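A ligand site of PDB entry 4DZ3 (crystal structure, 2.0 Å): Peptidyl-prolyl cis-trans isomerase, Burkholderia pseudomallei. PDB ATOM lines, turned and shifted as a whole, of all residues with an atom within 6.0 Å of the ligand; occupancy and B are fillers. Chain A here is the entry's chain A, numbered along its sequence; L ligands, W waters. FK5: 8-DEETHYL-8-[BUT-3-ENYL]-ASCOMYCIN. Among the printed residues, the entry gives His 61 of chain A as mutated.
The side-chain hydroxyl (OH) of Tyr 89 sits at hydrogen-bond distance from an oxygen (O3) of the ligand (2.7 Å). The backbone NH (N) of Ile 63 is in hydrogen-bond range of an oxygen (O2) of the ligand. O of His 61 is in hydrogen-bond range of O10 of the ligand (2.5 Å). The side-chain carboxylate (OD2) of Asp 44 sits at hydrogen-bond distance from an oxygen (O6) of the ligand (2.8 Å).
N of Gly 35 sits at hydrogen-bond distance from O of Asp 44. The side-chain hydroxyl of Tyr 33 lies within hydrogen-bond range of the side-chain carboxylate of Asp 44 (2.5 Å). OH of Tyr 33 sits at hydrogen-bond distance from NH1 of Arg 49 (2.8 Å). The side-chain carboxylate of Asp 44 lies within salt-bridge range of the guanidinium group of Arg 49. The backbone NH of Phe 43 lies within hydrogen-bond range of the backbone carbonyl oxygen of Gly 35 (2.9 Å). The backbone carbonyl oxygen (O) of Tyr 33 lies close to the side-chain hydroxyl (OG) of Ser 45 (3.4 Å).
Tyr 33 touches the ligand (CE1 to O4, 3.3 Å). Phe 43 touches the ligand. Arg 49 touches the ligand (NE to C44, 3.9 Å). Phe 53 touches the ligand (CE2 to C4, 3.4 Å). CA of Val 62 touches O2 of the ligand, at 3.2 Å. Trp 66 touches the ligand (CE2 to C3, 3.5 Å). O of Gly 88 touches C45 of the ligand (3.3 Å). CD1 of Ile 98 touches C35 of the ligand, at 3.8 Å. Phe 106 touches the ligand. Hydrophobic or aromatic side chains that line the ligand: Tyr 33, Phe 43, Phe 53, Val 62, Ile 63, Trp 66, Tyr 89, Ile 98 and Phe 106. Within 4 Å of the ligand: Tyr 33, Phe 43, Asp 44, Arg 49, Phe 53, His 61, Val 62, Ile 63, Trp 66, Gly 88, Tyr 89, Ile 98 and Phe 106. Along chain A the residues within 4 Å of the ligand span positions 33 to 106. The nearest printed residue that does not touch the ligand is Ala 94 (4.7 Å).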
ATOM      1  N   TYR A  33       7.343   5.542  -5.902  1.00  0.00           N
ATOM      2  CA  TYR A  33       6.802   6.883  -5.827  1.00  0.00           C
ATOM      3  C   TYR A  33       5.367   6.940  -6.214  1.00  0.00           C
ATOM      4  O   TYR A  33       4.875   6.063  -6.948  1.00  0.00           O
ATOM      5  CB  TYR A  33       7.599   7.852  -6.729  1.00  0.00           C
ATOM      6  CG  TYR A  33       7.360   7.654  -8.231  1.00  0.00           C
ATOM      7  CD1 TYR A  33       6.303   8.300  -8.894  1.00  0.00           C
ATOM      8  CD2 TYR A  33       8.181   6.803  -8.976  1.00  0.00           C
ATOM      9  CE1 TYR A  33       6.072   8.105 -10.241  1.00  0.00           C
ATOM     10  CE2 TYR A  33       7.975   6.608 -10.345  1.00  0.00           C
ATOM     11  CZ  TYR A  33       6.926   7.255 -10.968  1.00  0.00           C
ATOM     12  OH  TYR A  33       6.712   7.056 -12.301  1.00  0.00           O
ATOM     13  N   GLY A  35       2.844  10.316  -7.543  1.00  0.00           N
ATOM     14  CA  GLY A  35       2.804  11.711  -7.960  1.00  0.00           C
ATOM     15  C   GLY A  35       1.361  12.209  -8.067  1.00  0.00           C
ATOM     16  O   GLY A  35       0.491  11.520  -8.615  1.00  0.00           O
ATOM     17  N   PHE A  43      -1.440  11.385 -10.790  1.00  0.00           N
ATOM     18  CA  PHE A  43      -1.042  11.228 -12.226  1.00  0.00           C
ATOM     19  C   PHE A  43      -0.201   9.972 -12.494  1.00  0.00           C
ATOM     20  O   PHE A  43      -0.201   9.461 -13.613  1.00  0.00           O
ATOM     21  CB  PHE A  43      -0.354  12.500 -12.826  1.00  0.00           C
ATOM     22  CG  PHE A  43       0.897  12.978 -12.093  1.00  0.00           C
ATOM     23  CD1 PHE A  43       2.144  12.397 -12.341  1.00  0.00           C
ATOM     24  CD2 PHE A  43       0.815  14.035 -11.187  1.00  0.00           C
ATOM     25  CE1 PHE A  43       3.278  12.849 -11.682  1.00  0.00           C
ATOM     26  CE2 PHE A  43       1.941  14.494 -10.531  1.00  0.00           C
ATOM     27  CZ  PHE A  43       3.183  13.897 -10.763  1.00  0.00           C
ATOM     28  N   ASP A  44       0.508   9.465 -11.475  1.00  0.00           N
ATOM     29  CA  ASP A  44       1.315   8.262 -11.644  1.00  0.00           C
ATOM     30  C   ASP A  44       1.693   7.617 -10.310  1.00  0.00           C
ATOM     31  O   ASP A  44       1.751   8.290  -9.285  1.00  0.00           O
ATOM     32  CB  ASP A  44       2.612   8.585 -12.444  1.00  0.00           C
ATOM     33  CG  ASP A  44       3.340   7.336 -12.965  1.00  0.00           C
ATOM     34  OD1 ASP A  44       2.781   6.212 -12.910  1.00  0.00           O
ATOM     35  OD2 ASP A  44       4.491   7.468 -13.447  1.00  0.00           O
ATOM     36  N   SER A  45       1.918   6.306 -10.346  1.00  0.00           N
ATOM     37  CA  SER A  45       2.515   5.580  -9.234  1.00  0.00           C
ATOM     38  C   SER A  45       3.250   4.359  -9.727  1.00  0.00           C
ATOM     39  O   SER A  45       2.697   3.553 -10.502  1.00  0.00           O
ATOM     40  CB  SER A  45       1.452   5.165  -8.230  1.00  0.00           C
ATOM     41  OG  SER A  45       2.000   4.256  -7.267  1.00  0.00           O
ATOM     42  N   ARG A  49       2.196  -0.034 -11.183  1.00  0.00           N
ATOM     43  CA  ARG A  49       2.887  -0.830 -12.210  1.00  0.00           C
ATOM     44  C   ARG A  49       3.714  -1.995 -11.613  1.00  0.00           C
ATOM     45  O   ARG A  49       4.294  -2.806 -12.349  1.00  0.00           O
ATOM     46  CB  ARG A  49       3.809   0.082 -13.044  1.00  0.00           C
ATOM     47  CG  ARG A  49       3.054   1.113 -13.887  1.00  0.00           C
ATOM     48  CD  ARG A  49       3.972   1.961 -14.756  1.00  0.00           C
ATOM     49  NE  ARG A  49       4.388   3.191 -14.098  1.00  0.00           N
ATOM     50  CZ  ARG A  49       5.496   3.338 -13.383  1.00  0.00           C
ATOM     51  NH1 ARG A  49       5.784   4.499 -12.841  1.00  0.00           N
ATOM     52  NH2 ARG A  49       6.327   2.308 -13.227  1.00  0.00           N
ATOM     53  N   PHE A  53      11.477   2.241  -9.416  1.00  0.00           N
ATOM     54  CA  PHE A  53      12.099   3.171 -10.347  1.00  0.00           C
ATOM     55  C   PHE A  53      13.522   3.406  -9.905  1.00  0.00           C
ATOM     56  O   PHE A  53      13.744   3.829  -8.800  1.00  0.00           O
ATOM     57  CB  PHE A  53      11.307   4.497 -10.409  1.00  0.00           C
ATOM     58  CG  PHE A  53      11.979   5.576 -11.214  1.00  0.00           C
ATOM     59  CD1 PHE A  53      12.186   5.419 -12.586  1.00  0.00           C
ATOM     60  CD2 PHE A  53      12.419   6.756 -10.600  1.00  0.00           C
ATOM     61  CE1 PHE A  53      12.819   6.409 -13.335  1.00  0.00           C
ATOM     62  CE2 PHE A  53      13.037   7.757 -11.357  1.00  0.00           C
ATOM     63  CZ  PHE A  53      13.239   7.586 -12.712  1.00  0.00           C
ATOM     64  N   HIS A  61      18.630  13.090 -15.149  1.00  0.00           N
ATOM     65  CA  HIS A  61      17.637  12.345 -15.941  1.00  0.00           C
ATOM     66  C   HIS A  61      16.275  12.321 -15.325  1.00  0.00           C
ATOM     67  O   HIS A  61      15.407  11.590 -15.773  1.00  0.00           O
ATOM     68  CB  HIS A  61      18.172  10.963 -16.291  1.00  0.00           C
ATOM     69  CG  HIS A  61      19.059  11.018 -17.478  1.00  0.00           C
ATOM     70  ND1 HIS A  61      20.315  11.408 -17.394  1.00  0.00           N
ATOM     71  CD2 HIS A  61      18.797  10.784 -18.821  1.00  0.00           C
ATOM     72  CE1 HIS A  61      20.857  11.387 -18.616  1.00  0.00           C
ATOM     73  NE2 HIS A  61      19.912  11.003 -19.482  1.00  0.00           N
ATOM     74  N   VAL A  62      16.091  13.139 -14.295  1.00  0.00           N
ATOM     75  CA  VAL A  62      14.824  13.357 -13.645  1.00  0.00           C
ATOM     76  C   VAL A  62      14.651  14.841 -13.479  1.00  0.00           C
ATOM     77  O   VAL A  62      15.606  15.611 -13.600  1.00  0.00           O
ATOM     78  CB  VAL A  62      14.722  12.633 -12.263  1.00  0.00           C
ATOM     79  CG1 VAL A  62      14.721  11.110 -12.459  1.00  0.00           C
ATOM     80  CG2 VAL A  62      15.843  13.087 -11.297  1.00  0.00           C
ATOM     81  N   ILE A  63      13.435  15.262 -13.237  1.00  0.00           N
ATOM     82  CA  ILE A  63      13.152  16.689 -12.984  1.00  0.00           C
ATOM     83  C   ILE A  63      14.018  17.197 -11.789  1.00  0.00           C
ATOM     84  O   ILE A  63      14.377  16.415 -10.876  1.00  0.00           O
ATOM     85  CB  ILE A  63      11.629  16.957 -12.780  1.00  0.00           C
ATOM     86  CG1 ILE A  63      11.020  16.061 -11.683  1.00  0.00           C
ATOM     87  CG2 ILE A  63      10.874  16.777 -14.119  1.00  0.00           C
ATOM     88  CD1 ILE A  63       9.550  16.374 -11.409  1.00  0.00           C
ATOM     89  N   TRP A  66      13.496  16.284  -8.065  1.00  0.00           N
ATOM     90  CA  TRP A  66      13.919  14.921  -7.652  1.00  0.00           C
ATOM     91  C   TRP A  66      15.391  14.783  -7.382  1.00  0.00           C
ATOM     92  O   TRP A  66      15.796  14.214  -6.349  1.00  0.00           O
ATOM     93  CB  TRP A  66      13.542  13.885  -8.704  1.00  0.00           C
ATOM     94  CG  TRP A  66      12.196  13.318  -8.512  1.00  0.00           C
ATOM     95  CD1 TRP A  66      10.973  14.001  -8.517  1.00  0.00           C
ATOM     96  CD2 TRP A  66      11.867  11.943  -8.293  1.00  0.00           C
ATOM     97  NE1 TRP A  66       9.947  13.120  -8.309  1.00  0.00           N
ATOM     98  CE2 TRP A  66      10.427  11.871  -8.172  1.00  0.00           C
ATOM     99  CE3 TRP A  66      12.604  10.766  -8.194  1.00  0.00           C
ATOM    100  CZ2 TRP A  66       9.761  10.665  -7.963  1.00  0.00           C
ATOM    101  CZ3 TRP A  66      11.947   9.572  -7.984  1.00  0.00           C
ATOM    102  CH2 TRP A  66      10.551   9.521  -7.867  1.00  0.00           C
ATOM    103  N   GLY A  88      10.122  21.259 -12.030  1.00  0.00           N
ATOM    104  CA  GLY A  88       9.292  20.176 -12.567  1.00  0.00           C
ATOM    105  C   GLY A  88       9.271  20.276 -14.095  1.00  0.00           C
ATOM    106  O   GLY A  88      10.325  20.191 -14.736  1.00  0.00           O
ATOM    107  N   TYR A  89       8.077  20.468 -14.667  1.00  0.00           N
ATOM    108  CA  TYR A  89       7.881  20.524 -16.148  1.00  0.00           C
ATOM    109  C   TYR A  89       7.659  21.934 -16.690  1.00  0.00           C
ATOM    110  O   TYR A  89       7.327  22.105 -17.875  1.00  0.00           O
ATOM    111  CB  TYR A  89       6.738  19.569 -16.558  1.00  0.00           C
ATOM    112  CG  TYR A  89       7.101  18.149 -16.216  1.00  0.00           C
ATOM    113  CD1 TYR A  89       7.935  17.406 -17.045  1.00  0.00           C
ATOM    114  CD2 TYR A  89       6.634  17.548 -15.050  1.00  0.00           C
ATOM    115  CE1 TYR A  89       8.299  16.091 -16.737  1.00  0.00           C
ATOM    116  CE2 TYR A  89       6.992  16.218 -14.726  1.00  0.00           C
ATOM    117  CZ  TYR A  89       7.829  15.510 -15.591  1.00  0.00           C
ATOM    118  OH  TYR A  89       8.226  14.218 -15.345  1.00  0.00           O
ATOM    119  N   GLY A  90       7.831  22.943 -15.833  1.00  0.00           N
ATOM    120  CA  GLY A  90       7.760  24.327 -16.258  1.00  0.00           C
ATOM    121  C   GLY A  90       6.480  24.658 -16.992  1.00  0.00           C
ATOM    122  O   GLY A  90       5.407  24.149 -16.642  1.00  0.00           O
ATOM    123  N   ALA A  94       3.528  18.118 -19.304  1.00  0.00           N
ATOM    124  CA  ALA A  94       3.824  16.844 -19.960  1.00  0.00           C
ATOM    125  C   ALA A  94       2.534  16.251 -20.480  1.00  0.00           C
ATOM    126  O   ALA A  94       1.762  15.670 -19.702  1.00  0.00           O
ATOM    127  CB  ALA A  94       4.523  15.896 -18.984  1.00  0.00           C
ATOM    128  N   VAL A  97      -1.030  14.577 -18.958  1.00  0.00           N
ATOM    129  CA  VAL A  97      -0.813  14.137 -17.558  1.00  0.00           C
ATOM    130  C   VAL A  97      -0.600  15.349 -16.641  1.00  0.00           C
ATOM    131  O   VAL A  97      -1.290  15.486 -15.627  1.00  0.00           O
ATOM    132  CB  VAL A  97       0.409  13.205 -17.430  1.00  0.00           C
ATOM    133  N   ILE A  98       0.345  16.209 -16.994  1.00  0.00           N
ATOM    134  CA  ILE A  98       0.708  17.363 -16.174  1.00  0.00           C
ATOM    135  C   ILE A  98       0.474  18.665 -16.966  1.00  0.00           C
ATOM    136  O   ILE A  98       1.064  18.844 -18.011  1.00  0.00           O
ATOM    137  CB  ILE A  98       2.163  17.244 -15.701  1.00  0.00           C
ATOM    138  CG1 ILE A  98       2.324  15.939 -14.872  1.00  0.00           C
ATOM    139  CG2 ILE A  98       2.589  18.484 -14.883  1.00  0.00           C
ATOM    140  CD1 ILE A  98       3.696  15.700 -14.299  1.00  0.00           C
ATOM    141  N   LEU A 104       3.902  20.145  -8.317  1.00  0.00           N
ATOM    142  CA  LEU A 104       3.768  18.673  -8.211  1.00  0.00           C
ATOM    143  C   LEU A 104       4.021  18.226  -6.813  1.00  0.00           C
ATOM    144  O   LEU A 104       4.899  18.780  -6.130  1.00  0.00           O
ATOM    145  CB  LEU A 104       4.781  17.965  -9.137  1.00  0.00           C
ATOM    146  CG  LEU A 104       4.750  18.381 -10.606  1.00  0.00           C
ATOM    147  CD1 LEU A 104       5.838  17.647 -11.395  1.00  0.00           C
ATOM    148  CD2 LEU A 104       3.375  18.129 -11.203  1.00  0.00           C
ATOM    149  N   PHE A 106       5.036  14.769  -4.815  1.00  0.00           N
ATOM    150  CA  PHE A 106       5.420  13.364  -4.856  1.00  0.00           C
ATOM    151  C   PHE A 106       5.645  12.841  -3.460  1.00  0.00           C
ATOM    152  O   PHE A 106       6.119  13.584  -2.587  1.00  0.00           O
ATOM    153  CB  PHE A 106       6.733  13.162  -5.606  1.00  0.00           C
ATOM    154  CG  PHE A 106       6.642  13.361  -7.085  1.00  0.00           C
ATOM    155  CD1 PHE A 106       6.811  14.607  -7.639  1.00  0.00           C
ATOM    156  CD2 PHE A 106       6.436  12.271  -7.939  1.00  0.00           C
ATOM    157  CE1 PHE A 106       6.752  14.804  -9.023  1.00  0.00           C
ATOM    158  CE2 PHE A 106       6.374  12.454  -9.337  1.00  0.00           C
ATOM    159  CZ  PHE A 106       6.534  13.722  -9.867  1.00  0.00           C
HETATM  160  C1  FK5 L   1      10.730  12.419 -14.057  1.00  0.00           C
HETATM  161  C2  FK5 L   1       9.779  12.272 -12.905  1.00  0.00           C
HETATM  162  C3  FK5 L   1      10.536  11.892 -11.651  1.00  0.00           C
HETATM  163  C4  FK5 L   1      10.987  10.460 -11.595  1.00  0.00           C
HETATM  164  C5  FK5 L   1       9.766   9.580 -11.727  1.00  0.00           C
HETATM  165  C6  FK5 L   1       9.122   9.842 -13.065  1.00  0.00           C
HETATM  166  C8  FK5 L   1       7.399  11.748 -13.264  1.00  0.00           C
HETATM  167  C9  FK5 L   1       6.270  10.823 -13.462  1.00  0.00           C
HETATM  168  C10 FK5 L   1       5.833  10.360 -14.846  1.00  0.00           C
HETATM  169  C11 FK5 L   1       5.979  11.370 -15.992  1.00  0.00           C
HETATM  170  C12 FK5 L   1       5.850  10.672 -17.379  1.00  0.00           C
HETATM  171  C13 FK5 L   1       6.814   9.475 -17.479  1.00  0.00           C
HETATM  172  C14 FK5 L   1       6.515   8.536 -16.292  1.00  0.00           C
HETATM  173  C15 FK5 L   1       7.370   7.247 -16.140  1.00  0.00           C
HETATM  174  C16 FK5 L   1       8.893   7.514 -16.163  1.00  0.00           C
HETATM  175  C17 FK5 L   1       9.792   6.294 -15.773  1.00  0.00           C
HETATM  176  C18 FK5 L   1      10.017   5.288 -16.928  1.00  0.00           C
HETATM  177  C19 FK5 L   1      11.036   5.843 -17.875  1.00  0.00           C
HETATM  178  C20 FK5 L   1      10.627   6.547 -18.942  1.00  0.00           C
HETATM  179  C21 FK5 L   1      11.572   7.157 -19.954  1.00  0.00           C
HETATM  180  C22 FK5 L   1      11.676   8.625 -19.614  1.00  0.00           C
HETATM  181  C23 FK5 L   1      12.897   9.071 -18.840  1.00  0.00           C
HETATM  182  C24 FK5 L   1      12.717  10.425 -18.137  1.00  0.00           C
HETATM  183  C25 FK5 L   1      11.752  10.407 -16.923  1.00  0.00           C
HETATM  184  C26 FK5 L   1      11.476  11.800 -16.320  1.00  0.00           C
HETATM  185  C27 FK5 L   1      10.922  12.743 -17.329  1.00  0.00           C
HETATM  186  C28 FK5 L   1      11.667  13.861 -17.616  1.00  0.00           C
HETATM  187  C29 FK5 L   1      11.265  14.904 -18.622  1.00  0.00           C
HETATM  188  C30 FK5 L   1      11.627  16.302 -18.121  1.00  0.00           C
HETATM  189  C31 FK5 L   1      11.483  17.400 -19.193  1.00  0.00           C
HETATM  190  C32 FK5 L   1      12.131  17.034 -20.528  1.00  0.00           C
HETATM  191  C33 FK5 L   1      11.847  15.605 -20.989  1.00  0.00           C
HETATM  192  C34 FK5 L   1      11.995  14.555 -19.909  1.00  0.00           C
HETATM  193  C35 FK5 L   1       5.001  12.519 -15.796  1.00  0.00           C
HETATM  194  C36 FK5 L   1       9.237   5.534 -14.555  1.00  0.00           C
HETATM  195  C37 FK5 L   1      12.478   5.568 -17.559  1.00  0.00           C
HETATM  196  C38 FK5 L   1      11.046   6.906 -21.354  1.00  0.00           C
HETATM  197  C39 FK5 L   1      11.711   7.866 -22.299  1.00  0.00           C
HETATM  198  C40 FK5 L   1      12.887   7.662 -22.823  1.00  0.00           C
HETATM  199  C41 FK5 L   1      12.292   9.522 -15.823  1.00  0.00           C
HETATM  200  C42 FK5 L   1       9.596  12.399 -17.976  1.00  0.00           C
HETATM  201  C43 FK5 L   1       7.272   9.447 -19.844  1.00  0.00           C
HETATM  202  C44 FK5 L   1       5.791   5.575 -16.824  1.00  0.00           C
HETATM  203  C45 FK5 L   1      11.414  19.297 -17.665  1.00  0.00           C
HETATM  204  N7  FK5 L   1       8.661  11.262 -13.092  1.00  0.00           N
HETATM  205  O1  FK5 L   1      10.528  11.649 -15.265  1.00  0.00           O
HETATM  206  O2  FK5 L   1      11.660  13.202 -13.938  1.00  0.00           O
HETATM  207  O3  FK5 L   1       7.120  12.941 -13.239  1.00  0.00           O
HETATM  208  O4  FK5 L   1       5.665  10.450 -12.462  1.00  0.00           O
HETATM  209  O5  FK5 L   1       6.697   9.259 -15.090  1.00  0.00           O
HETATM  210  O6  FK5 L   1       4.453   9.954 -14.779  1.00  0.00           O
HETATM  211  O7  FK5 L   1       6.712   8.766 -18.718  1.00  0.00           O
HETATM  212  O8  FK5 L   1       6.986   6.318 -17.153  1.00  0.00           O
HETATM  213  O9  FK5 L   1      10.816   9.426 -19.950  1.00  0.00           O
HETATM  214  O10 FK5 L   1      14.007  10.850 -17.707  1.00  0.00           O
HETATM  215  O11 FK5 L   1      12.114  18.619 -18.726  1.00  0.00           O
HETATM  216  O12 FK5 L   1      11.601  17.889 -21.527  1.00  0.00           O
HETATM  217  O   HOH W   1       7.145   5.775 -20.017  1.00  0.00           O
